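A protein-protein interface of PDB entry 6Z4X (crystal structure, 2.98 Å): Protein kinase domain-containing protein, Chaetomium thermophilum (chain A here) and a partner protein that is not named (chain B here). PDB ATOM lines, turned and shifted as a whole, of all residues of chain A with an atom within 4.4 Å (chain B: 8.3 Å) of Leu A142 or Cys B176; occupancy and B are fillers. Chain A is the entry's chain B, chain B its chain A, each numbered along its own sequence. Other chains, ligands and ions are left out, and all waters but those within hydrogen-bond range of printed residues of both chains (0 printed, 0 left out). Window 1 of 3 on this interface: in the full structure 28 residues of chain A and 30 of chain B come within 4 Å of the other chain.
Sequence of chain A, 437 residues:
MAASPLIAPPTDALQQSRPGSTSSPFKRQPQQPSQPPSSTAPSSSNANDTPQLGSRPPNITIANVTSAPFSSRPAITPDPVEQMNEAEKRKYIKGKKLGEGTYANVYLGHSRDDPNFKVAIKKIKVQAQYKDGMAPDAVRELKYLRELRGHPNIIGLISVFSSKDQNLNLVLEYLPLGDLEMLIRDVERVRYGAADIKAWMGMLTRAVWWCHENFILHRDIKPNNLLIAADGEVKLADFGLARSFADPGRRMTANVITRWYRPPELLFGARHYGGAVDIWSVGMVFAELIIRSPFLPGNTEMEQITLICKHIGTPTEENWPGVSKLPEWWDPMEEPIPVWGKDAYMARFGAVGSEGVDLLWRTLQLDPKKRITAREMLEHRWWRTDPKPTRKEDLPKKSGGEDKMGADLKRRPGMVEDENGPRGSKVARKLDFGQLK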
ATOM      1  N   MET A 134      36.428  20.708   5.804  1.00  0.00           N
ATOM      2  CA  MET A 134      35.401  21.575   5.240  1.00  0.00           C
ATOM      3  C   MET A 134      35.919  23.001   5.073  1.00  0.00           C
ATOM      4  O   MET A 134      36.562  23.558   5.966  1.00  0.00           O
ATOM      5  CB  MET A 134      34.157  21.559   6.126  1.00  0.00           C
ATOM      6  CG  MET A 134      32.931  22.181   5.487  1.00  0.00           C
ATOM      7  SD  MET A 134      31.445  21.795   6.428  1.00  0.00           S
ATOM      8  CE  MET A 134      31.624  20.019   6.604  1.00  0.00           C
ATOM      9  N   ALA A 138      32.212  27.489   3.397  1.00  0.00           N
ATOM     10  CA  ALA A 138      31.074  26.602   3.609  1.00  0.00           C
ATOM     11  C   ALA A 138      30.559  26.702   5.040  1.00  0.00           C
ATOM     12  O   ALA A 138      29.356  26.885   5.269  1.00  0.00           O
ATOM     13  CB  ALA A 138      31.468  25.162   3.276  1.00  0.00           C
ATOM     14  N   VAL A 139      31.461  26.589   6.020  1.00  0.00           N
ATOM     15  CA  VAL A 139      31.059  26.689   7.421  1.00  0.00           C
ATOM     16  C   VAL A 139      30.443  28.052   7.703  1.00  0.00           C
ATOM     17  O   VAL A 139      29.411  28.160   8.379  1.00  0.00           O
ATOM     18  CB  VAL A 139      32.263  26.412   8.342  1.00  0.00           C
ATOM     19  CG1 VAL A 139      31.896  26.687   9.790  1.00  0.00           C
ATOM     20  CG2 VAL A 139      32.746  24.980   8.169  1.00  0.00           C
ATOM     21  N   ARG A 140      31.075  29.116   7.203  1.00  0.00           N
ATOM     22  CA  ARG A 140      30.601  30.466   7.482  1.00  0.00           C
ATOM     23  C   ARG A 140      29.195  30.678   6.938  1.00  0.00           C
ATOM     24  O   ARG A 140      28.329  31.233   7.626  1.00  0.00           O
ATOM     25  CB  ARG A 140      31.578  31.490   6.903  1.00  0.00           C
ATOM     26  CG  ARG A 140      32.830  31.640   7.738  1.00  0.00           C
ATOM     27  CD  ARG A 140      33.944  32.365   7.013  1.00  0.00           C
ATOM     28  NE  ARG A 140      35.071  32.597   7.913  1.00  0.00           N
ATOM     29  CZ  ARG A 140      36.327  32.771   7.519  1.00  0.00           C
ATOM     30  NH1 ARG A 140      36.635  32.731   6.228  1.00  0.00           N
ATOM     31  NH2 ARG A 140      37.281  32.972   8.420  1.00  0.00           N
ATOM     32  N   GLU A 141      28.951  30.258   5.695  1.00  0.00           N
ATOM     33  CA  GLU A 141      27.601  30.352   5.157  1.00  0.00           C
ATOM     34  C   GLU A 141      26.632  29.531   5.998  1.00  0.00           C
ATOM     35  O   GLU A 141      25.616  30.050   6.475  1.00  0.00           O
ATOM     36  CB  GLU A 141      27.581  29.907   3.693  1.00  0.00           C
ATOM     37  CG  GLU A 141      28.345  30.840   2.762  1.00  0.00           C
ATOM     38  CD  GLU A 141      27.655  31.043   1.422  1.00  0.00           C
ATOM     39  OE1 GLU A 141      27.045  30.081   0.911  1.00  0.00           O
ATOM     40  OE2 GLU A 141      27.722  32.169   0.881  1.00  0.00           O
ATOM     41  N   LEU A 142      26.961  28.257   6.238  1.00  0.00           N
ATOM     42  CA  LEU A 142      26.065  27.380   6.987  1.00  0.00           C
ATOM     43  C   LEU A 142      25.670  27.984   8.328  1.00  0.00           C
ATOM     44  O   LEU A 142      24.542  27.792   8.798  1.00  0.00           O
ATOM     45  CB  LEU A 142      26.729  26.020   7.196  1.00  0.00           C
ATOM     46  CG  LEU A 142      25.767  24.843   7.335  1.00  0.00           C
ATOM     47  CD1 LEU A 142      24.796  24.826   6.171  1.00  0.00           C
ATOM     48  CD2 LEU A 142      26.538  23.533   7.413  1.00  0.00           C
ATOM     49  N   LYS A 143      26.587  28.707   8.965  1.00  0.00           N
ATOM     50  CA  LYS A 143      26.293  29.317  10.258  1.00  0.00           C
ATOM     51  C   LYS A 143      25.467  30.593  10.095  1.00  0.00           C
ATOM     52  O   LYS A 143      24.359  30.720  10.641  1.00  0.00           O
ATOM     53  CB  LYS A 143      27.612  29.603  10.989  1.00  0.00           C
ATOM     54  CG  LYS A 143      27.498  30.287  12.344  1.00  0.00           C
ATOM     55  CD  LYS A 143      28.886  30.646  12.869  1.00  0.00           C
ATOM     56  CE  LYS A 143      28.827  31.387  14.194  1.00  0.00           C
ATOM     57  NZ  LYS A 143      30.164  31.918  14.594  1.00  0.00           N
ATOM     58  N   TYR A 144      25.985  31.546   9.323  1.00  0.00           N
ATOM     59  CA  TYR A 144      25.445  32.897   9.360  1.00  0.00           C
ATOM     60  C   TYR A 144      24.193  33.057   8.505  1.00  0.00           C
ATOM     61  O   TYR A 144      23.310  33.842   8.868  1.00  0.00           O
ATOM     62  CB  TYR A 144      26.538  33.886   8.959  1.00  0.00           C
ATOM     63  CG  TYR A 144      27.699  33.859   9.929  1.00  0.00           C
ATOM     64  CD1 TYR A 144      27.476  33.940  11.301  1.00  0.00           C
ATOM     65  CD2 TYR A 144      29.009  33.733   9.487  1.00  0.00           C
ATOM     66  CE1 TYR A 144      28.524  33.911  12.203  1.00  0.00           C
ATOM     67  CE2 TYR A 144      30.066  33.706  10.385  1.00  0.00           C
ATOM     68  CZ  TYR A 144      29.815  33.794  11.741  1.00  0.00           C
ATOM     69  OH  TYR A 144      30.858  33.762  12.638  1.00  0.00           O
ATOM     70  N   ARG A 146      21.912  30.949   8.385  1.00  0.00           N
ATOM     71  CA  ARG A 146      20.889  30.544   9.342  1.00  0.00           C
ATOM     72  C   ARG A 146      20.677  31.615  10.401  1.00  0.00           C
ATOM     73  O   ARG A 146      19.537  31.892  10.792  1.00  0.00           O
ATOM     74  CB  ARG A 146      21.271  29.219  10.002  1.00  0.00           C
ATOM     75  CG  ARG A 146      20.337  28.813  11.132  1.00  0.00           C
ATOM     76  CD  ARG A 146      18.905  28.658  10.647  1.00  0.00           C
ATOM     77  NE  ARG A 146      17.972  28.462  11.753  1.00  0.00           N
ATOM     78  CZ  ARG A 146      17.410  29.454  12.438  1.00  0.00           C
ATOM     79  NH1 ARG A 146      17.687  30.715  12.132  1.00  0.00           N
ATOM     80  NH2 ARG A 146      16.571  29.188  13.430  1.00  0.00           N
ATOM     81  N   VAL A 160      18.835  22.898   4.560  1.00  0.00           N
ATOM     82  CA  VAL A 160      20.180  22.346   4.415  1.00  0.00           C
ATOM     83  C   VAL A 160      20.093  20.831   4.518  1.00  0.00           C
ATOM     84  O   VAL A 160      19.400  20.305   5.396  1.00  0.00           O
ATOM     85  CB  VAL A 160      21.152  22.898   5.478  1.00  0.00           C
ATOM     86  CG1 VAL A 160      22.520  22.248   5.328  1.00  0.00           C
ATOM     87  CG2 VAL A 160      21.255  24.410   5.369  1.00  0.00           C
ATOM     88  N   LEU A 168      27.402  18.660   0.715  1.00  0.00           N
ATOM     89  CA  LEU A 168      26.539  19.628   1.375  1.00  0.00           C
ATOM     90  C   LEU A 168      25.637  20.295   0.345  1.00  0.00           C
ATOM     91  O   LEU A 168      26.076  20.615  -0.764  1.00  0.00           O
ATOM     92  CB  LEU A 168      27.380  20.675   2.108  1.00  0.00           C
ATOM     93  CG  LEU A 168      26.702  21.570   3.144  1.00  0.00           C
ATOM     94  CD1 LEU A 168      26.110  20.726   4.265  1.00  0.00           C
ATOM     95  CD2 LEU A 168      27.700  22.570   3.706  1.00  0.00           C
ATOM     96  N   LEU A 170      22.555  23.375   0.011  1.00  0.00           N
ATOM     97  CA  LEU A 170      21.816  24.499   0.571  1.00  0.00           C
ATOM     98  C   LEU A 170      20.636  24.821  -0.336  1.00  0.00           C
ATOM     99  O   LEU A 170      20.826  25.173  -1.505  1.00  0.00           O
ATOM    100  CB  LEU A 170      22.721  25.722   0.716  1.00  0.00           C
ATOM    101  CG  LEU A 170      24.041  25.503   1.455  1.00  0.00           C
ATOM    102  CD1 LEU A 170      24.805  26.809   1.588  1.00  0.00           C
ATOM    103  CD2 LEU A 170      23.799  24.877   2.817  1.00  0.00           C
ATOM    104  N   SER B  16      18.424  28.961  15.800  1.00  0.00           N
ATOM    105  CA  SER B  16      18.456  27.525  15.552  1.00  0.00           C
ATOM    106  C   SER B  16      18.522  26.748  16.857  1.00  0.00           C
ATOM    107  O   SER B  16      17.938  25.665  16.973  1.00  0.00           O
ATOM    108  CB  SER B  16      19.648  27.166  14.665  1.00  0.00           C
ATOM    109  OG  SER B  16      20.868  27.374  15.354  1.00  0.00           O
ATOM    110  N   TRP B  21      17.531  22.438  19.126  1.00  0.00           N
ATOM    111  CA  TRP B  21      18.200  21.790  20.247  1.00  0.00           C
ATOM    112  C   TRP B  21      17.715  22.363  21.571  1.00  0.00           C
ATOM    113  O   TRP B  21      18.508  22.676  22.465  1.00  0.00           O
ATOM    114  CB  TRP B  21      19.715  21.914  20.116  1.00  0.00           C
ATOM    115  CG  TRP B  21      20.251  21.337  18.835  1.00  0.00           C
ATOM    116  CD1 TRP B  21      20.704  22.029  17.748  1.00  0.00           C
ATOM    117  CD2 TRP B  21      20.378  19.950  18.508  1.00  0.00           C
ATOM    118  NE1 TRP B  21      21.111  21.156  16.767  1.00  0.00           N
ATOM    119  CE2 TRP B  21      20.919  19.874  17.209  1.00  0.00           C
ATOM    120  CE3 TRP B  21      20.087  18.762  19.187  1.00  0.00           C
ATOM    121  CZ2 TRP B  21      21.174  18.660  16.580  1.00  0.00           C
ATOM    122  CZ3 TRP B  21      20.341  17.560  18.558  1.00  0.00           C
ATOM    123  CH2 TRP B  21      20.880  17.517  17.269  1.00  0.00           C
ATOM    124  N   PHE B 117      28.486  20.510  20.433  1.00  0.00           N
ATOM    125  CA  PHE B 117      28.458  19.655  19.250  1.00  0.00           C
ATOM    126  C   PHE B 117      28.526  18.186  19.639  1.00  0.00           C
ATOM    127  O   PHE B 117      27.817  17.351  19.067  1.00  0.00           O
ATOM    128  CB  PHE B 117      29.616  20.007  18.313  1.00  0.00           C
ATOM    129  CG  PHE B 117      29.440  21.310  17.585  1.00  0.00           C
ATOM    130  CD1 PHE B 117      28.207  21.939  17.545  1.00  0.00           C
ATOM    131  CD2 PHE B 117      30.513  21.905  16.940  1.00  0.00           C
ATOM    132  CE1 PHE B 117      28.050  23.138  16.875  1.00  0.00           C
ATOM    133  CE2 PHE B 117      30.360  23.100  16.269  1.00  0.00           C
ATOM    134  CZ  PHE B 117      29.129  23.718  16.237  1.00  0.00           C
ATOM    135  N   PHE B 121      25.556  15.587  18.829  1.00  0.00           N
ATOM    136  CA  PHE B 121      25.818  14.440  17.973  1.00  0.00           C
ATOM    137  C   PHE B 121      25.425  13.145  18.664  1.00  0.00           C
ATOM    138  O   PHE B 121      24.865  12.242  18.032  1.00  0.00           O
ATOM    139  CB  PHE B 121      27.289  14.395  17.566  1.00  0.00           C
ATOM    140  CG  PHE B 121      27.633  13.211  16.707  1.00  0.00           C
ATOM    141  CD1 PHE B 121      27.440  13.256  15.336  1.00  0.00           C
ATOM    142  CD2 PHE B 121      28.118  12.042  17.274  1.00  0.00           C
ATOM    143  CE1 PHE B 121      27.740  12.167  14.545  1.00  0.00           C
ATOM    144  CE2 PHE B 121      28.418  10.948  16.487  1.00  0.00           C
ATOM    145  CZ  PHE B 121      28.229  11.012  15.121  1.00  0.00           C
ATOM    146  N   THR B 124      21.569  12.736  18.837  1.00  0.00           N
ATOM    147  CA  THR B 124      21.020  12.245  17.573  1.00  0.00           C
ATOM    148  C   THR B 124      21.652  10.936  17.110  1.00  0.00           C
ATOM    149  O   THR B 124      21.070  10.247  16.262  1.00  0.00           O
ATOM    150  CB  THR B 124      21.180  13.294  16.471  1.00  0.00           C
ATOM    151  OG1 THR B 124      22.537  13.745  16.442  1.00  0.00           O
ATOM    152  CG2 THR B 124      20.265  14.476  16.730  1.00  0.00           C
ATOM    153  N   ASN B 125      22.818  10.578  17.643  1.00  0.00           N
ATOM    154  CA  ASN B 125      23.480   9.320  17.326  1.00  0.00           C
ATOM    155  C   ASN B 125      23.793   8.571  18.613  1.00  0.00           C
ATOM    156  O   ASN B 125      23.884   9.159  19.695  1.00  0.00           O
ATOM    157  CB  ASN B 125      24.771   9.531  16.517  1.00  0.00           C
ATOM    158  CG  ASN B 125      24.511  10.084  15.128  1.00  0.00           C
ATOM    159  OD1 ASN B 125      24.314   9.330  14.175  1.00  0.00           O
ATOM    160  ND2 ASN B 125      24.521  11.405  15.005  1.00  0.00           N
ATOM    161  N   MET B 135      35.216  11.131  18.092  1.00  0.00           N
ATOM    162  CA  MET B 135      34.281  12.234  17.933  1.00  0.00           C
ATOM    163  C   MET B 135      34.582  13.374  18.894  1.00  0.00           C
ATOM    164  O   MET B 135      34.196  14.511  18.623  1.00  0.00           O
ATOM    165  CB  MET B 135      32.848  11.735  18.113  1.00  0.00           C
ATOM    166  CG  MET B 135      32.434  10.748  17.035  1.00  0.00           C
ATOM    167  SD  MET B 135      32.748  11.398  15.377  1.00  0.00           S
ATOM    168  CE  MET B 135      32.417   9.951  14.375  1.00  0.00           C
ATOM    169  N   VAL B 138      36.960  15.316  16.901  1.00  0.00           N
ATOM    170  CA  VAL B 138      36.210  15.838  15.760  1.00  0.00           C
ATOM    171  C   VAL B 138      35.397  17.058  16.177  1.00  0.00           C
ATOM    172  O   VAL B 138      35.348  18.069  15.464  1.00  0.00           O
ATOM    173  CB  VAL B 138      35.315  14.746  15.148  1.00  0.00           C
ATOM    174  CG1 VAL B 138      34.481  15.325  14.015  1.00  0.00           C
ATOM    175  CG2 VAL B 138      36.155  13.583  14.658  1.00  0.00           C
ATOM    176  N   PHE B 142      35.712  20.877  14.751  1.00  0.00           N
ATOM    177  CA  PHE B 142      34.599  21.560  14.107  1.00  0.00           C
ATOM    178  C   PHE B 142      34.122  22.746  14.934  1.00  0.00           C
ATOM    179  O   PHE B 142      33.593  23.708  14.376  1.00  0.00           O
ATOM    180  CB  PHE B 142      33.450  20.588  13.845  1.00  0.00           C
ATOM    181  CG  PHE B 142      32.524  21.039  12.751  1.00  0.00           C
ATOM    182  CD1 PHE B 142      32.989  21.180  11.453  1.00  0.00           C
ATOM    183  CD2 PHE B 142      31.195  21.328  13.016  1.00  0.00           C
ATOM    184  CE1 PHE B 142      32.147  21.598  10.439  1.00  0.00           C
ATOM    185  CE2 PHE B 142      30.346  21.747  12.004  1.00  0.00           C
ATOM    186  CZ  PHE B 142      30.824  21.881  10.715  1.00  0.00           C
ATOM    187  N   GLY B 171      35.583  12.204  10.409  1.00  0.00           N
ATOM    188  CA  GLY B 171      34.365  12.406  11.166  1.00  0.00           C
ATOM    189  C   GLY B 171      33.710  13.749  10.918  1.00  0.00           C
ATOM    190  O   GLY B 171      32.512  13.911  11.173  1.00  0.00           O
ATOM    191  N   GLU B 172      34.471  14.705  10.379  1.00  0.00           N
ATOM    192  CA  GLU B 172      34.006  16.084  10.311  1.00  0.00           C
ATOM    193  C   GLU B 172      32.605  16.162   9.718  1.00  0.00           C
ATOM    194  O   GLU B 172      31.643  16.459  10.434  1.00  0.00           O
ATOM    195  CB  GLU B 172      34.973  16.954   9.502  1.00  0.00           C
ATOM    196  CG  GLU B 172      34.643  18.442   9.583  1.00  0.00           C
ATOM    197  CD  GLU B 172      35.606  19.309   8.799  1.00  0.00           C
ATOM    198  OE1 GLU B 172      35.953  20.404   9.291  1.00  0.00           O
ATOM    199  OE2 GLU B 172      36.028  18.894   7.697  1.00  0.00           O
ATOM    200  N   PHE B 173      32.472  15.867   8.422  1.00  0.00           N
ATOM    201  CA  PHE B 173      31.165  15.971   7.786  1.00  0.00           C
ATOM    202  C   PHE B 173      30.121  15.159   8.540  1.00  0.00           C
ATOM    203  O   PHE B 173      28.978  15.603   8.707  1.00  0.00           O
ATOM    204  CB  PHE B 173      31.244  15.515   6.329  1.00  0.00           C
ATOM    205  CG  PHE B 173      30.016  15.846   5.526  1.00  0.00           C
ATOM    206  CD1 PHE B 173      29.671  17.166   5.278  1.00  0.00           C
ATOM    207  CD2 PHE B 173      29.205  14.840   5.028  1.00  0.00           C
ATOM    208  CE1 PHE B 173      28.543  17.475   4.542  1.00  0.00           C
ATOM    209  CE2 PHE B 173      28.074  15.144   4.290  1.00  0.00           C
ATOM    210  CZ  PHE B 173      27.745  16.464   4.047  1.00  0.00           C
ATOM    211  N   LEU B 174      30.504  13.977   9.031  1.00  0.00           N
ATOM    212  CA  LEU B 174      29.568  13.166   9.802  1.00  0.00           C
ATOM    213  C   LEU B 174      29.007  13.962  10.972  1.00  0.00           C
ATOM    214  O   LEU B 174      27.787  14.077  11.135  1.00  0.00           O
ATOM    215  CB  LEU B 174      30.255  11.891  10.292  1.00  0.00           C
ATOM    216  CG  LEU B 174      29.373  10.906  11.057  1.00  0.00           C
ATOM    217  CD1 LEU B 174      28.267  10.373  10.161  1.00  0.00           C
ATOM    218  CD2 LEU B 174      30.211   9.765  11.615  1.00  0.00           C
ATOM    219  N   LEU B 175      29.893  14.546  11.781  1.00  0.00           N
ATOM    220  CA  LEU B 175      29.445  15.389  12.881  1.00  0.00           C
ATOM    221  C   LEU B 175      28.511  16.486  12.384  1.00  0.00           C
ATOM    222  O   LEU B 175      27.501  16.793  13.029  1.00  0.00           O
ATOM    223  CB  LEU B 175      30.650  15.996  13.596  1.00  0.00           C
ATOM    224  CG  LEU B 175      30.353  17.054  14.657  1.00  0.00           C
ATOM    225  CD1 LEU B 175      29.559  16.447  15.808  1.00  0.00           C
ATOM    226  CD2 LEU B 175      31.647  17.680  15.158  1.00  0.00           C
ATOM    227  N   CYS B 176      28.827  17.079  11.230  1.00  0.00           N
ATOM    228  CA  CYS B 176      27.981  18.139  10.693  1.00  0.00           C
ATOM    229  C   CYS B 176      26.556  17.649  10.503  1.00  0.00           C
ATOM    230  O   CYS B 176      25.595  18.369  10.798  1.00  0.00           O
ATOM    231  CB  CYS B 176      28.548  18.648   9.370  1.00  0.00           C
ATOM    232  SG  CYS B 176      27.937  20.284   8.894  1.00  0.00           S
ATOM    233  N   GLN B 177      26.402  16.414  10.019  1.00  0.00           N
ATOM    234  CA  GLN B 177      25.067  15.855   9.862  1.00  0.00           C
ATOM    235  C   GLN B 177      24.414  15.620  11.213  1.00  0.00           C
ATOM    236  O   GLN B 177      23.202  15.805  11.363  1.00  0.00           O
ATOM    237  CB  GLN B 177      25.124  14.554   9.062  1.00  0.00           C
ATOM    238  CG  GLN B 177      25.784  14.703   7.706  1.00  0.00           C
ATOM    239  CD  GLN B 177      25.903  13.391   6.951  1.00  0.00           C
ATOM    240  OE1 GLN B 177      25.157  13.139   6.001  1.00  0.00           O
ATOM    241  NE2 GLN B 177      26.847  12.554   7.359  1.00  0.00           N
ATOM    242  N   GLY B 178      25.205  15.213  12.206  1.00  0.00           N
ATOM    243  CA  GLY B 178      24.636  14.856  13.495  1.00  0.00           C
ATOM    244  C   GLY B 178      23.986  16.026  14.206  1.00  0.00           C
ATOM    245  O   GLY B 178      22.935  15.877  14.832  1.00  0.00           O
ATOM    246  N   ILE B 179      24.600  17.205  14.124  1.00  0.00           N
ATOM    247  CA  ILE B 179      24.099  18.378  14.829  1.00  0.00           C
ATOM    248  C   ILE B 179      23.016  19.061  14.005  1.00  0.00           C
ATOM    249  O   ILE B 179      22.543  20.148  14.357  1.00  0.00           O
ATOM    250  CB  ILE B 179      25.245  19.351  15.157  1.00  0.00           C
ATOM    251  CG1 ILE B 179      25.912  19.848  13.873  1.00  0.00           C
ATOM    252  CG2 ILE B 179      26.267  18.676  16.056  1.00  0.00           C
ATOM    253  CD1 ILE B 179      26.995  20.878  14.109  1.00  0.00           C
ATOM    254  N   ARG B 180      22.612  18.425  12.906  1.00  0.00           N
ATOM    255  CA  ARG B 180      21.571  18.953  12.024  1.00  0.00           C
ATOM    256  C   ARG B 180      21.935  20.341  11.496  1.00  0.00           C
ATOM    257  O   ARG B 180      21.081  21.216  11.342  1.00  0.00           O
ATOM    258  CB  ARG B 180      20.206  18.960  12.717  1.00  0.00           C
ATOM    259  CG  ARG B 180      19.604  17.565  12.867  1.00  0.00           C
ATOM    260  CD  ARG B 180      18.122  17.590  13.230  1.00  0.00           C
ATOM    261  NE  ARG B 180      17.907  17.622  14.676  1.00  0.00           N
ATOM    262  CZ  ARG B 180      16.712  17.616  15.258  1.00  0.00           C
ATOM    263  NH1 ARG B 180      16.613  17.649  16.582  1.00  0.00           N
ATOM    264  NH2 ARG B 180      15.614  17.565  14.517  1.00  0.00           N
ATOM    265  N   PHE B 181      23.223  20.537  11.209  1.00  0.00           N
ATOM    266  CA  PHE B 181      23.732  21.703  10.490  1.00  0.00           C
ATOM    267  C   PHE B 181      23.512  23.014  11.238  1.00  0.00           C
ATOM    268  O   PHE B 181      23.525  24.087  10.625  1.00  0.00           O
ATOM    269  CB  PHE B 181      23.121  21.783   9.088  1.00  0.00           C
ATOM    270  CG  PHE B 181      23.278  20.519   8.293  1.00  0.00           C
ATOM    271  CD1 PHE B 181      24.440  20.274   7.581  1.00  0.00           C
ATOM    272  CD2 PHE B 181      22.271  19.568   8.270  1.00  0.00           C
ATOM    273  CE1 PHE B 181      24.592  19.109   6.850  1.00  0.00           C
ATOM    274  CE2 PHE B 181      22.417  18.400   7.542  1.00  0.00           C
ATOM    275  CZ  PHE B 181      23.579  18.171   6.831  1.00  0.00           C
ATOM    276  N   ALA B 182      23.311  22.962  12.552  1.00  0.00           N
ATOM    277  CA  ALA B 182      23.159  24.163  13.374  1.00  0.00           C
ATOM    278  C   ALA B 182      24.521  24.495  13.971  1.00  0.00           C
ATOM    279  O   ALA B 182      24.982  23.830  14.903  1.00  0.00           O
ATOM    280  CB  ALA B 182      22.104  23.956  14.456  1.00  0.00           C
ATOM    281  N   LEU B 183      25.171  25.527  13.428  1.00  0.00           N
ATOM    282  CA  LEU B 183      26.509  25.913  13.859  1.00  0.00           C
ATOM    283  C   LEU B 183      26.530  27.131  14.776  1.00  0.00           C
ATOM    284  O   LEU B 183      27.566  27.398  15.396  1.00  0.00           O
ATOM    285  CB  LEU B 183      27.404  26.180  12.641  1.00  0.00           C
ATOM    286  CG  LEU B 183      28.028  24.945  11.987  1.00  0.00           C
ATOM    287  CD1 LEU B 183      26.973  23.890  11.697  1.00  0.00           C
ATOM    288  CD2 LEU B 183      28.775  25.322  10.716  1.00  0.00           C
ATOM    289  N   ASP B 184      25.430  27.871  14.881  1.00  0.00           N
ATOM    290  CA  ASP B 184      25.385  29.075  15.710  1.00  0.00           C
ATOM    291  C   ASP B 184      24.931  28.670  17.106  1.00  0.00           C
ATOM    292  O   ASP B 184      23.744  28.439  17.346  1.00  0.00           O
ATOM    293  CB  ASP B 184      24.461  30.123  15.099  1.00  0.00           C
ATOM    294  CG  ASP B 184      23.051  29.613  14.890  1.00  0.00           C
ATOM    295  OD1 ASP B 184      22.890  28.433  14.510  1.00  0.00           O
ATOM    296  OD2 ASP B 184      22.102  30.395  15.112  1.00  0.00           O
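Of the 12 printed residues of chain A, 7 touch a printed residue of chain B.
Of the 23 printed residues of chain B, 6 touch a printed residue of chain A.
Printed residues of chain B that touch a printed residue of chain A: Ser B16, Glu B172, Phe B173, Cys B176, Phe B181 and Leu B183.
Hydrophobic or aromatic side chains of chain B that line the printed part of chain A: Phe B173, Phe B181 and Leu B183.
Leu A142 touches just these residues of chain B: Cys B176 (3.8 Å) and Phe B181 (3.9 Å).
Of the printed residues of chain B, Val A160 touches Phe B181.
Of the printed residues of chain A, Ser B16 touches Arg A146 (3.0 Å).
Phe B142 touches none of the printed residues of chain A.
Printed residues of chain A within 4 Å of Phe B173: Met A134.
Of chain A, only Leu A142 (3.8 Å) comes within 4 Å of Cys B176.
Ala B182 touches none of the printed residues of chain A.
Printed residues of chain A within 4 Å of Leu B183: Val A139 and Lys A143.
The side-chain carboxylate (OE2) of Glu B172 sits at hydrogen-bond distance from the backbone NH (N) of Met A134 (2.7 Å).
The backbone NH of Ser B16 sits close to the guanidinium group of Arg A146 (3.0 Å).
The side-chain hydroxyl (OG) of Ser B16 sits at hydrogen-bond distance from the side-chain carboxylate (OD1) of Asp B184, 2.4 Å away.
N of Phe B181 lies within hydrogen-bond range of O of Cys B176.
OH of Tyr A144 sits at hydrogen-bond distance from NZ of Lys A143, at 2.8 Å.
Among the printed residues, pairs that only touch across the chains: Leu A168 with Phe B181, Val A160 with Phe B181, Val A139 with Leu B183, Met A134 with Phe B173, Lys A143 with Leu B183, Leu A142 with Cys B176 and Leu A142 with Phe B181.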
